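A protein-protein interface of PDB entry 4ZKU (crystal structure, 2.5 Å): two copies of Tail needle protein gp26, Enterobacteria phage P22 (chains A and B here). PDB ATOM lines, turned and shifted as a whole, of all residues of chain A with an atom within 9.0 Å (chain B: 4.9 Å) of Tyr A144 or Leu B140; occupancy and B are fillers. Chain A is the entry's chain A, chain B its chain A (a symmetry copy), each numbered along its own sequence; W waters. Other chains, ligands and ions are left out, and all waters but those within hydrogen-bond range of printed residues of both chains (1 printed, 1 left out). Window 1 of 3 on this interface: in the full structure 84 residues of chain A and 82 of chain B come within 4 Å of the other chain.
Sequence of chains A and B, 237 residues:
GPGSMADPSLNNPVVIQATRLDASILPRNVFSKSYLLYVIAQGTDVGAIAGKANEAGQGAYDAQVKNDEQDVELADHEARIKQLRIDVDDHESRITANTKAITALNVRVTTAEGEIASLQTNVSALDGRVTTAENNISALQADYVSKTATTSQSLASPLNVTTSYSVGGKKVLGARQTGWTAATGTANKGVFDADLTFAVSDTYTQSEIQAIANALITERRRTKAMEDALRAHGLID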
ATOM      1  N   ALA A 133      -6.859 -19.999  -9.634  1.00  0.00           N
ATOM      2  CA  ALA A 133      -6.701 -18.654 -10.172  1.00  0.00           C
ATOM      3  C   ALA A 133      -5.238 -18.363 -10.492  1.00  0.00           C
ATOM      4  O   ALA A 133      -4.930 -17.779 -11.528  1.00  0.00           O
ATOM      5  CB  ALA A 133      -7.246 -17.624  -9.195  1.00  0.00           C
ATOM      6  N   GLU A 134      -4.342 -18.781  -9.601  1.00  0.00           N
ATOM      7  CA  GLU A 134      -2.909 -18.584  -9.804  1.00  0.00           C
ATOM      8  C   GLU A 134      -2.404 -19.302 -11.051  1.00  0.00           C
ATOM      9  O   GLU A 134      -1.498 -18.819 -11.728  1.00  0.00           O
ATOM     10  CB  GLU A 134      -2.118 -19.056  -8.579  1.00  0.00           C
ATOM     11  CG  GLU A 134      -2.280 -18.172  -7.352  1.00  0.00           C
ATOM     12  CD  GLU A 134      -1.504 -18.687  -6.155  1.00  0.00           C
ATOM     13  OE1 GLU A 134      -0.968 -17.858  -5.389  1.00  0.00           O
ATOM     14  OE2 GLU A 134      -1.450 -19.921  -5.967  1.00  0.00           O
ATOM     15  N   ASN A 136      -4.356 -20.050 -13.686  1.00  0.00           N
ATOM     16  CA  ASN A 136      -4.985 -19.383 -14.820  1.00  0.00           C
ATOM     17  C   ASN A 136      -4.226 -18.108 -15.163  1.00  0.00           C
ATOM     18  O   ASN A 136      -4.100 -17.737 -16.330  1.00  0.00           O
ATOM     19  CB  ASN A 136      -6.447 -19.049 -14.514  1.00  0.00           C
ATOM     20  CG  ASN A 136      -7.350 -20.261 -14.580  1.00  0.00           C
ATOM     21  OD1 ASN A 136      -7.093 -21.205 -15.328  1.00  0.00           O
ATOM     22  ND2 ASN A 136      -8.420 -20.241 -13.794  1.00  0.00           N
ATOM     23  N   ILE A 137      -3.723 -17.445 -14.129  1.00  0.00           N
ATOM     24  CA  ILE A 137      -2.938 -16.232 -14.293  1.00  0.00           C
ATOM     25  C   ILE A 137      -1.610 -16.576 -14.964  1.00  0.00           C
ATOM     26  O   ILE A 137      -1.161 -15.872 -15.869  1.00  0.00           O
ATOM     27  CB  ILE A 137      -2.737 -15.528 -12.941  1.00  0.00           C
ATOM     28  CG1 ILE A 137      -4.063 -14.947 -12.446  1.00  0.00           C
ATOM     29  CG2 ILE A 137      -1.733 -14.415 -13.067  1.00  0.00           C
ATOM     30  CD1 ILE A 137      -3.956 -14.215 -11.126  1.00  0.00           C
ATOM     31  N   SER A 138      -0.984 -17.659 -14.511  1.00  0.00           N
ATOM     32  CA  SER A 138       0.286 -18.108 -15.072  1.00  0.00           C
ATOM     33  C   SER A 138       0.121 -18.444 -16.551  1.00  0.00           C
ATOM     34  O   SER A 138       0.981 -18.126 -17.374  1.00  0.00           O
ATOM     35  CB  SER A 138       0.816 -19.326 -14.314  1.00  0.00           C
ATOM     36  OG  SER A 138       1.329 -18.958 -13.047  1.00  0.00           O
ATOM     37  N   ALA A 139      -0.993 -19.093 -16.875  1.00  0.00           N
ATOM     38  CA  ALA A 139      -1.302 -19.470 -18.249  1.00  0.00           C
ATOM     39  C   ALA A 139      -1.522 -18.236 -19.121  1.00  0.00           C
ATOM     40  O   ALA A 139      -1.082 -18.196 -20.268  1.00  0.00           O
ATOM     41  CB  ALA A 139      -2.524 -20.377 -18.287  1.00  0.00           C
ATOM     42  N   LEU A 140      -2.202 -17.237 -18.571  1.00  0.00           N
ATOM     43  CA  LEU A 140      -2.461 -15.995 -19.287  1.00  0.00           C
ATOM     44  C   LEU A 140      -1.178 -15.202 -19.523  1.00  0.00           C
ATOM     45  O   LEU A 140      -1.015 -14.565 -20.561  1.00  0.00           O
ATOM     46  CB  LEU A 140      -3.474 -15.137 -18.524  1.00  0.00           C
ATOM     47  CG  LEU A 140      -4.951 -15.512 -18.668  1.00  0.00           C
ATOM     48  CD1 LEU A 140      -5.757 -14.995 -17.486  1.00  0.00           C
ATOM     49  CD2 LEU A 140      -5.524 -14.996 -19.978  1.00  0.00           C
ATOM     50  N   GLN A 141      -0.273 -15.242 -18.553  1.00  0.00           N
ATOM     51  CA  GLN A 141       0.960 -14.471 -18.628  1.00  0.00           C
ATOM     52  C   GLN A 141       1.877 -15.004 -19.720  1.00  0.00           C
ATOM     53  O   GLN A 141       2.554 -14.238 -20.401  1.00  0.00           O
ATOM     54  CB  GLN A 141       1.689 -14.491 -17.285  1.00  0.00           C
ATOM     55  CG  GLN A 141       1.023 -13.666 -16.198  1.00  0.00           C
ATOM     56  CD  GLN A 141       1.752 -13.757 -14.873  1.00  0.00           C
ATOM     57  OE1 GLN A 141       1.575 -12.914 -13.997  1.00  0.00           O
ATOM     58  NE2 GLN A 141       2.575 -14.785 -14.719  1.00  0.00           N
ATOM     59  N   ALA A 142       1.897 -16.322 -19.876  1.00  0.00           N
ATOM     60  CA  ALA A 142       2.761 -16.961 -20.858  1.00  0.00           C
ATOM     61  C   ALA A 142       2.200 -16.797 -22.266  1.00  0.00           C
ATOM     62  O   ALA A 142       2.944 -16.800 -23.242  1.00  0.00           O
ATOM     63  CB  ALA A 142       2.946 -18.432 -20.525  1.00  0.00           C
ATOM     64  N   ASP A 143       0.884 -16.650 -22.360  1.00  0.00           N
ATOM     65  CA  ASP A 143       0.178 -16.847 -23.620  1.00  0.00           C
ATOM     66  C   ASP A 143      -0.382 -15.568 -24.249  1.00  0.00           C
ATOM     67  O   ASP A 143      -0.716 -15.556 -25.434  1.00  0.00           O
ATOM     68  CB  ASP A 143      -0.957 -17.850 -23.401  1.00  0.00           C
ATOM     69  CG  ASP A 143      -1.553 -18.353 -24.698  1.00  0.00           C
ATOM     70  OD1 ASP A 143      -0.782 -18.764 -25.591  1.00  0.00           O
ATOM     71  OD2 ASP A 143      -2.795 -18.344 -24.822  1.00  0.00           O
ATOM     72  N   TYR A 144      -0.483 -14.494 -23.472  1.00  0.00           N
ATOM     73  CA  TYR A 144      -1.155 -13.284 -23.951  1.00  0.00           C
ATOM     74  C   TYR A 144      -0.229 -12.372 -24.755  1.00  0.00           C
ATOM     75  O   TYR A 144       0.989 -12.393 -24.577  1.00  0.00           O
ATOM     76  CB  TYR A 144      -1.752 -12.507 -22.775  1.00  0.00           C
ATOM     77  CG  TYR A 144      -0.803 -11.525 -22.127  1.00  0.00           C
ATOM     78  CD1 TYR A 144       0.253 -11.963 -21.339  1.00  0.00           C
ATOM     79  CD2 TYR A 144      -0.971 -10.156 -22.295  1.00  0.00           C
ATOM     80  CE1 TYR A 144       1.120 -11.066 -20.741  1.00  0.00           C
ATOM     81  CE2 TYR A 144      -0.110  -9.252 -21.702  1.00  0.00           C
ATOM     82  CZ  TYR A 144       0.933  -9.712 -20.926  1.00  0.00           C
ATOM     83  OH  TYR A 144       1.792  -8.814 -20.335  1.00  0.00           O
ATOM     84  N   VAL A 145      -0.822 -11.568 -25.634  1.00  0.00           N
ATOM     85  CA  VAL A 145      -0.074 -10.615 -26.447  1.00  0.00           C
ATOM     86  C   VAL A 145       0.006  -9.273 -25.726  1.00  0.00           C
ATOM     87  O   VAL A 145      -1.016  -8.700 -25.346  1.00  0.00           O
ATOM     88  CB  VAL A 145      -0.706 -10.452 -27.841  1.00  0.00           C
ATOM     89  CG1 VAL A 145       0.054  -9.412 -28.654  1.00  0.00           C
ATOM     90  CG2 VAL A 145      -0.733 -11.787 -28.565  1.00  0.00           C
ATOM     91  N   SER A 146       1.225  -8.776 -25.546  1.00  0.00           N
ATOM     92  CA  SER A 146       1.462  -7.582 -24.738  1.00  0.00           C
ATOM     93  C   SER A 146       1.529  -6.295 -25.558  1.00  0.00           C
ATOM     94  O   SER A 146       2.052  -6.280 -26.672  1.00  0.00           O
ATOM     95  CB  SER A 146       2.755  -7.746 -23.937  1.00  0.00           C
ATOM     96  OG  SER A 146       3.138  -6.523 -23.332  1.00  0.00           O
ATOM     97  N   LYS A 147       0.990  -5.218 -24.992  1.00  0.00           N
ATOM     98  CA  LYS A 147       1.044  -3.901 -25.620  1.00  0.00           C
ATOM     99  C   LYS A 147       2.403  -3.236 -25.418  1.00  0.00           C
ATOM    100  O   LYS A 147       2.781  -2.340 -26.174  1.00  0.00           O
ATOM    101  CB  LYS A 147      -0.053  -2.989 -25.062  1.00  0.00           C
ATOM    102  CG  LYS A 147      -1.473  -3.373 -25.450  1.00  0.00           C
ATOM    103  CD  LYS A 147      -2.470  -2.367 -24.893  1.00  0.00           C
ATOM    104  CE  LYS A 147      -3.904  -2.778 -25.183  1.00  0.00           C
ATOM    105  NZ  LYS A 147      -4.887  -1.879 -24.512  1.00  0.00           N
ATOM    106  N   THR A 148       3.134  -3.671 -24.395  1.00  0.00           N
ATOM    107  CA  THR A 148       4.345  -2.972 -23.978  1.00  0.00           C
ATOM    108  C   THR A 148       5.624  -3.765 -24.240  1.00  0.00           C
ATOM    109  O   THR A 148       6.720  -3.206 -24.195  1.00  0.00           O
ATOM    110  CB  THR A 148       4.294  -2.614 -22.479  1.00  0.00           C
ATOM    111  OG1 THR A 148       3.988  -3.786 -21.714  1.00  0.00           O
ATOM    112  CG2 THR A 148       3.236  -1.553 -22.221  1.00  0.00           C
ATOM    113  N   ALA A 149       5.486  -5.062 -24.502  1.00  0.00           N
ATOM    114  CA  ALA A 149       6.641  -5.899 -24.814  1.00  0.00           C
ATOM    115  C   ALA A 149       7.338  -5.380 -26.067  1.00  0.00           C
ATOM    116  O   ALA A 149       6.683  -4.920 -27.001  1.00  0.00           O
ATOM    117  CB  ALA A 149       6.221  -7.347 -24.997  1.00  0.00           C
ATOM    118  N   GLN A 153       6.517 -10.564 -31.167  1.00  0.00           N
ATOM    119  CA  GLN A 153       5.559 -11.552 -30.688  1.00  0.00           C
ATOM    120  C   GLN A 153       4.929 -12.283 -31.868  1.00  0.00           C
ATOM    121  O   GLN A 153       4.615 -11.672 -32.889  1.00  0.00           O
ATOM    122  CB  GLN A 153       4.488 -10.884 -29.823  1.00  0.00           C
ATOM    123  CG  GLN A 153       5.051  -9.843 -28.865  1.00  0.00           C
ATOM    124  CD  GLN A 153       3.999  -9.253 -27.946  1.00  0.00           C
ATOM    125  OE1 GLN A 153       3.374  -9.967 -27.160  1.00  0.00           O
ATOM    126  NE2 GLN A 153       3.801  -7.942 -28.035  1.00  0.00           N
ATOM    127  N   SER A 154       4.750 -13.592 -31.727  1.00  0.00           N
ATOM    128  CA  SER A 154       4.296 -14.417 -32.841  1.00  0.00           C
ATOM    129  C   SER A 154       3.008 -15.170 -32.517  1.00  0.00           C
ATOM    130  O   SER A 154       2.867 -15.745 -31.438  1.00  0.00           O
ATOM    131  CB  SER A 154       5.391 -15.407 -33.247  1.00  0.00           C
ATOM    132  OG  SER A 154       4.973 -16.211 -34.337  1.00  0.00           O
ATOM    133  N   LEU A 155       2.073 -15.161 -33.463  1.00  0.00           N
ATOM    134  CA  LEU A 155       0.828 -15.908 -33.322  1.00  0.00           C
ATOM    135  C   LEU A 155       0.875 -17.198 -34.131  1.00  0.00           C
ATOM    136  O   LEU A 155       1.479 -17.251 -35.203  1.00  0.00           O
ATOM    137  CB  LEU A 155      -0.372 -15.068 -33.770  1.00  0.00           C
ATOM    138  CG  LEU A 155      -0.560 -13.661 -33.202  1.00  0.00           C
ATOM    139  CD1 LEU A 155      -1.877 -13.074 -33.691  1.00  0.00           C
ATOM    140  CD2 LEU A 155      -0.514 -13.682 -31.686  1.00  0.00           C
ATOM    141  N   ASN B 136      -1.328  -8.991 -10.491  1.00  0.00           N
ATOM    142  CA  ASN B 136      -1.037  -9.646 -11.761  1.00  0.00           C
ATOM    143  C   ASN B 136      -2.198  -9.452 -12.727  1.00  0.00           C
ATOM    144  O   ASN B 136      -2.004  -9.302 -13.934  1.00  0.00           O
ATOM    145  CB  ASN B 136      -0.776 -11.140 -11.558  1.00  0.00           C
ATOM    146  CG  ASN B 136       0.590 -11.419 -10.969  1.00  0.00           C
ATOM    147  OD1 ASN B 136       1.540 -10.667 -11.183  1.00  0.00           O
ATOM    148  ND2 ASN B 136       0.695 -12.512 -10.222  1.00  0.00           N
ATOM    149  N   ILE B 137      -3.406  -9.456 -12.178  1.00  0.00           N
ATOM    150  CA  ILE B 137      -4.614  -9.244 -12.960  1.00  0.00           C
ATOM    151  C   ILE B 137      -4.640  -7.803 -13.468  1.00  0.00           C
ATOM    152  O   ILE B 137      -4.966  -7.550 -14.629  1.00  0.00           O
ATOM    153  CB  ILE B 137      -5.864  -9.587 -12.134  1.00  0.00           C
ATOM    154  CG1 ILE B 137      -5.940 -11.096 -11.894  1.00  0.00           C
ATOM    155  CG2 ILE B 137      -7.111  -9.143 -12.848  1.00  0.00           C
ATOM    156  CD1 ILE B 137      -7.155 -11.530 -11.102  1.00  0.00           C
ATOM    157  N   SER B 138      -4.300  -6.863 -12.591  1.00  0.00           N
ATOM    158  CA  SER B 138      -4.269  -5.448 -12.949  1.00  0.00           C
ATOM    159  C   SER B 138      -3.259  -5.207 -14.066  1.00  0.00           C
ATOM    160  O   SER B 138      -3.512  -4.439 -14.995  1.00  0.00           O
ATOM    161  CB  SER B 138      -3.922  -4.587 -11.734  1.00  0.00           C
ATOM    162  OG  SER B 138      -5.016  -4.497 -10.839  1.00  0.00           O
ATOM    163  N   ALA B 139      -2.111  -5.870 -13.961  1.00  0.00           N
ATOM    164  CA  ALA B 139      -1.054  -5.758 -14.957  1.00  0.00           C
ATOM    165  C   ALA B 139      -1.500  -6.331 -16.300  1.00  0.00           C
ATOM    166  O   ALA B 139      -1.203  -5.765 -17.351  1.00  0.00           O
ATOM    167  CB  ALA B 139       0.208  -6.456 -14.471  1.00  0.00           C
ATOM    168  N   LEU B 140      -2.212  -7.451 -16.258  1.00  0.00           N
ATOM    169  CA  LEU B 140      -2.720  -8.088 -17.466  1.00  0.00           C
ATOM    170  C   LEU B 140      -3.796  -7.242 -18.141  1.00  0.00           C
ATOM    171  O   LEU B 140      -3.881  -7.194 -19.365  1.00  0.00           O
ATOM    172  CB  LEU B 140      -3.271  -9.480 -17.147  1.00  0.00           C
ATOM    173  CG  LEU B 140      -2.254 -10.614 -16.993  1.00  0.00           C
ATOM    174  CD1 LEU B 140      -2.829 -11.746 -16.157  1.00  0.00           C
ATOM    175  CD2 LEU B 140      -1.790 -11.124 -18.347  1.00  0.00           C
ATOM    176  N   GLN B 141      -4.617  -6.579 -17.334  1.00  0.00           N
ATOM    177  CA  GLN B 141      -5.729  -5.796 -17.855  1.00  0.00           C
ATOM    178  C   GLN B 141      -5.232  -4.572 -18.612  1.00  0.00           C
ATOM    179  O   GLN B 141      -5.811  -4.180 -19.622  1.00  0.00           O
ATOM    180  CB  GLN B 141      -6.657  -5.362 -16.721  1.00  0.00           C
ATOM    181  CG  GLN B 141      -7.488  -6.484 -16.127  1.00  0.00           C
ATOM    182  CD  GLN B 141      -8.354  -6.017 -14.975  1.00  0.00           C
ATOM    183  OE1 GLN B 141      -9.322  -6.677 -14.606  1.00  0.00           O
ATOM    184  NE2 GLN B 141      -8.007  -4.875 -14.399  1.00  0.00           N
ATOM    185  N   ALA B 142      -4.158  -3.969 -18.112  1.00  0.00           N
ATOM    186  CA  ALA B 142      -3.607  -2.767 -18.718  1.00  0.00           C
ATOM    187  C   ALA B 142      -2.836  -3.102 -19.989  1.00  0.00           C
ATOM    188  O   ALA B 142      -2.719  -2.275 -20.890  1.00  0.00           O
ATOM    189  CB  ALA B 142      -2.716  -2.036 -17.729  1.00  0.00           C
ATOM    190  N   ASP B 143      -2.313  -4.321 -20.055  1.00  0.00           N
ATOM    191  CA  ASP B 143      -1.266  -4.656 -21.012  1.00  0.00           C
ATOM    192  C   ASP B 143      -1.706  -5.592 -22.142  1.00  0.00           C
ATOM    193  O   ASP B 143      -1.021  -5.697 -23.160  1.00  0.00           O
ATOM    194  CB  ASP B 143      -0.088  -5.279 -20.261  1.00  0.00           C
ATOM    195  CG  ASP B 143       1.161  -5.381 -21.110  1.00  0.00           C
ATOM    196  OD1 ASP B 143       1.539  -4.373 -21.742  1.00  0.00           O
ATOM    197  OD2 ASP B 143       1.769  -6.471 -21.140  1.00  0.00           O
ATOM    198  N   TYR B 144      -2.841  -6.265 -21.976  1.00  0.00           N
ATOM    199  CA  TYR B 144      -3.245  -7.296 -22.934  1.00  0.00           C
ATOM    200  C   TYR B 144      -3.991  -6.724 -24.138  1.00  0.00           C
ATOM    201  O   TYR B 144      -4.606  -5.660 -24.054  1.00  0.00           O
ATOM    202  CB  TYR B 144      -4.111  -8.352 -22.243  1.00  0.00           C
ATOM    203  CG  TYR B 144      -5.588  -8.031 -22.216  1.00  0.00           C
ATOM    204  CD1 TYR B 144      -6.089  -7.035 -21.386  1.00  0.00           C
ATOM    205  CD2 TYR B 144      -6.485  -8.732 -23.013  1.00  0.00           C
ATOM    206  CE1 TYR B 144      -7.441  -6.743 -21.356  1.00  0.00           C
ATOM    207  CE2 TYR B 144      -7.838  -8.446 -22.990  1.00  0.00           C
ATOM    208  CZ  TYR B 144      -8.310  -7.452 -22.159  1.00  0.00           C
ATOM    209  OH  TYR B 144      -9.656  -7.165 -22.135  1.00  0.00           O
HETATM  210  O   HOH W   1       0.363 -10.093 -14.831  1.00  0.00           O
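OD2 of Asp B143 sits at hydrogen-bond distance from OH of Tyr A144 (2.5 Å).
The side-chain hydroxyl (OG) of Ser A146 sits at hydrogen-bond distance from the side-chain carboxylate (OD2) of Asp B143 (2.6 Å).
O of Asp B143 lies within hydrogen-bond range of N of Lys A147, at 2.8 Å.
The side-chain hydroxyl (OG1) of Thr A148 is in hydrogen-bond range of the side-chain carboxylate (OD1) of Asp B143, at 2.5 Å.
The side-chain hydroxyl (OG) of Ser A146 sits at hydrogen-bond distance from the backbone NH (N) of Thr A148.
OG of Ser A146 is in hydrogen-bond range of N of Ala A149, at 3.0 Å.
The side-chain amide nitrogen (NE2) of Gln A153 sits at hydrogen-bond distance from the backbone carbonyl oxygen (O) of Ser A146.
CB of Asn B136 touches CG2 of Ile A137, 3.7 Å away.
Ile A137 touches Ile B137 (CD1 to CG1, 3.8 Å).
Gln A141 touches Asn B136 (OE1 to CG, 3.5 Å).
Leu B140 touches Tyr A144.
Tyr A144 touches Tyr B144.
O of Val A145 touches O of Asp B143, at 3.7 Å.
Val A145 touches Tyr B144.
O of Tyr B144 touches CE of Lys A147 (3.2 Å).
Tyr A144 touches just these residues of chain B: Leu B140 (3.7 Å), Asp B143 (2.5 Å) and Tyr B144 (3.6 Å).
No residue of chain A comes within 4 Å of Ala B139.
Printed residues of chain A within 4 Å of Asn B136: Ile A137 (3.7 Å) and Gln A141 (3.5 Å).
Of the printed residues of chain B, Ser A146 touches Asp B143.
Printed residues of chain B within 4 Å of Gln A141: Asn B136.
Ala A149 touches none of the printed residues of chain B.
The nearest residue of chain A that does not touch Leu B140 is Leu A140 (4.2 Å).
Printed residues of chain A that touch a printed residue of chain B: Ile A137, Gln A141, Tyr A144, Val A145, Ser A146, Lys A147 and Thr A148.
Hydrophobic or aromatic side chains of chain A within 4 Å of the printed part of chain B: Ile A137 and Tyr A144.
Along chain A the printed residues that touch a printed residue of chain B span positions 137 to 148.
Of the 9 printed residues of chain B, 5 touch a printed residue of chain A.
Printed residues of chain B that touch a printed residue of chain A: Asn B136, Ile B137, Leu B140, Asp B143 and Tyr B144.
Among the printed residues, 12 pairs touch across the chains.
Ile A137 touches Asn B136, but with the chains exchanged Asn A136 does not touch Ile B137 (7.9 Å).
Ile A137 touches its own counterpart, Ile B137.
Tyr A144 touches Leu B140, but with the chains exchanged Leu A140 does not touch Tyr B144 (7.0 Å).
Tyr A144 touches Asp B143, but with the chains exchanged Asp A143 does not touch Tyr B144 (8.4 Å).
Water W1 bridges O of Asn B136 (2.7 Å) and OE1 of Gln A141 (3.2 Å).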
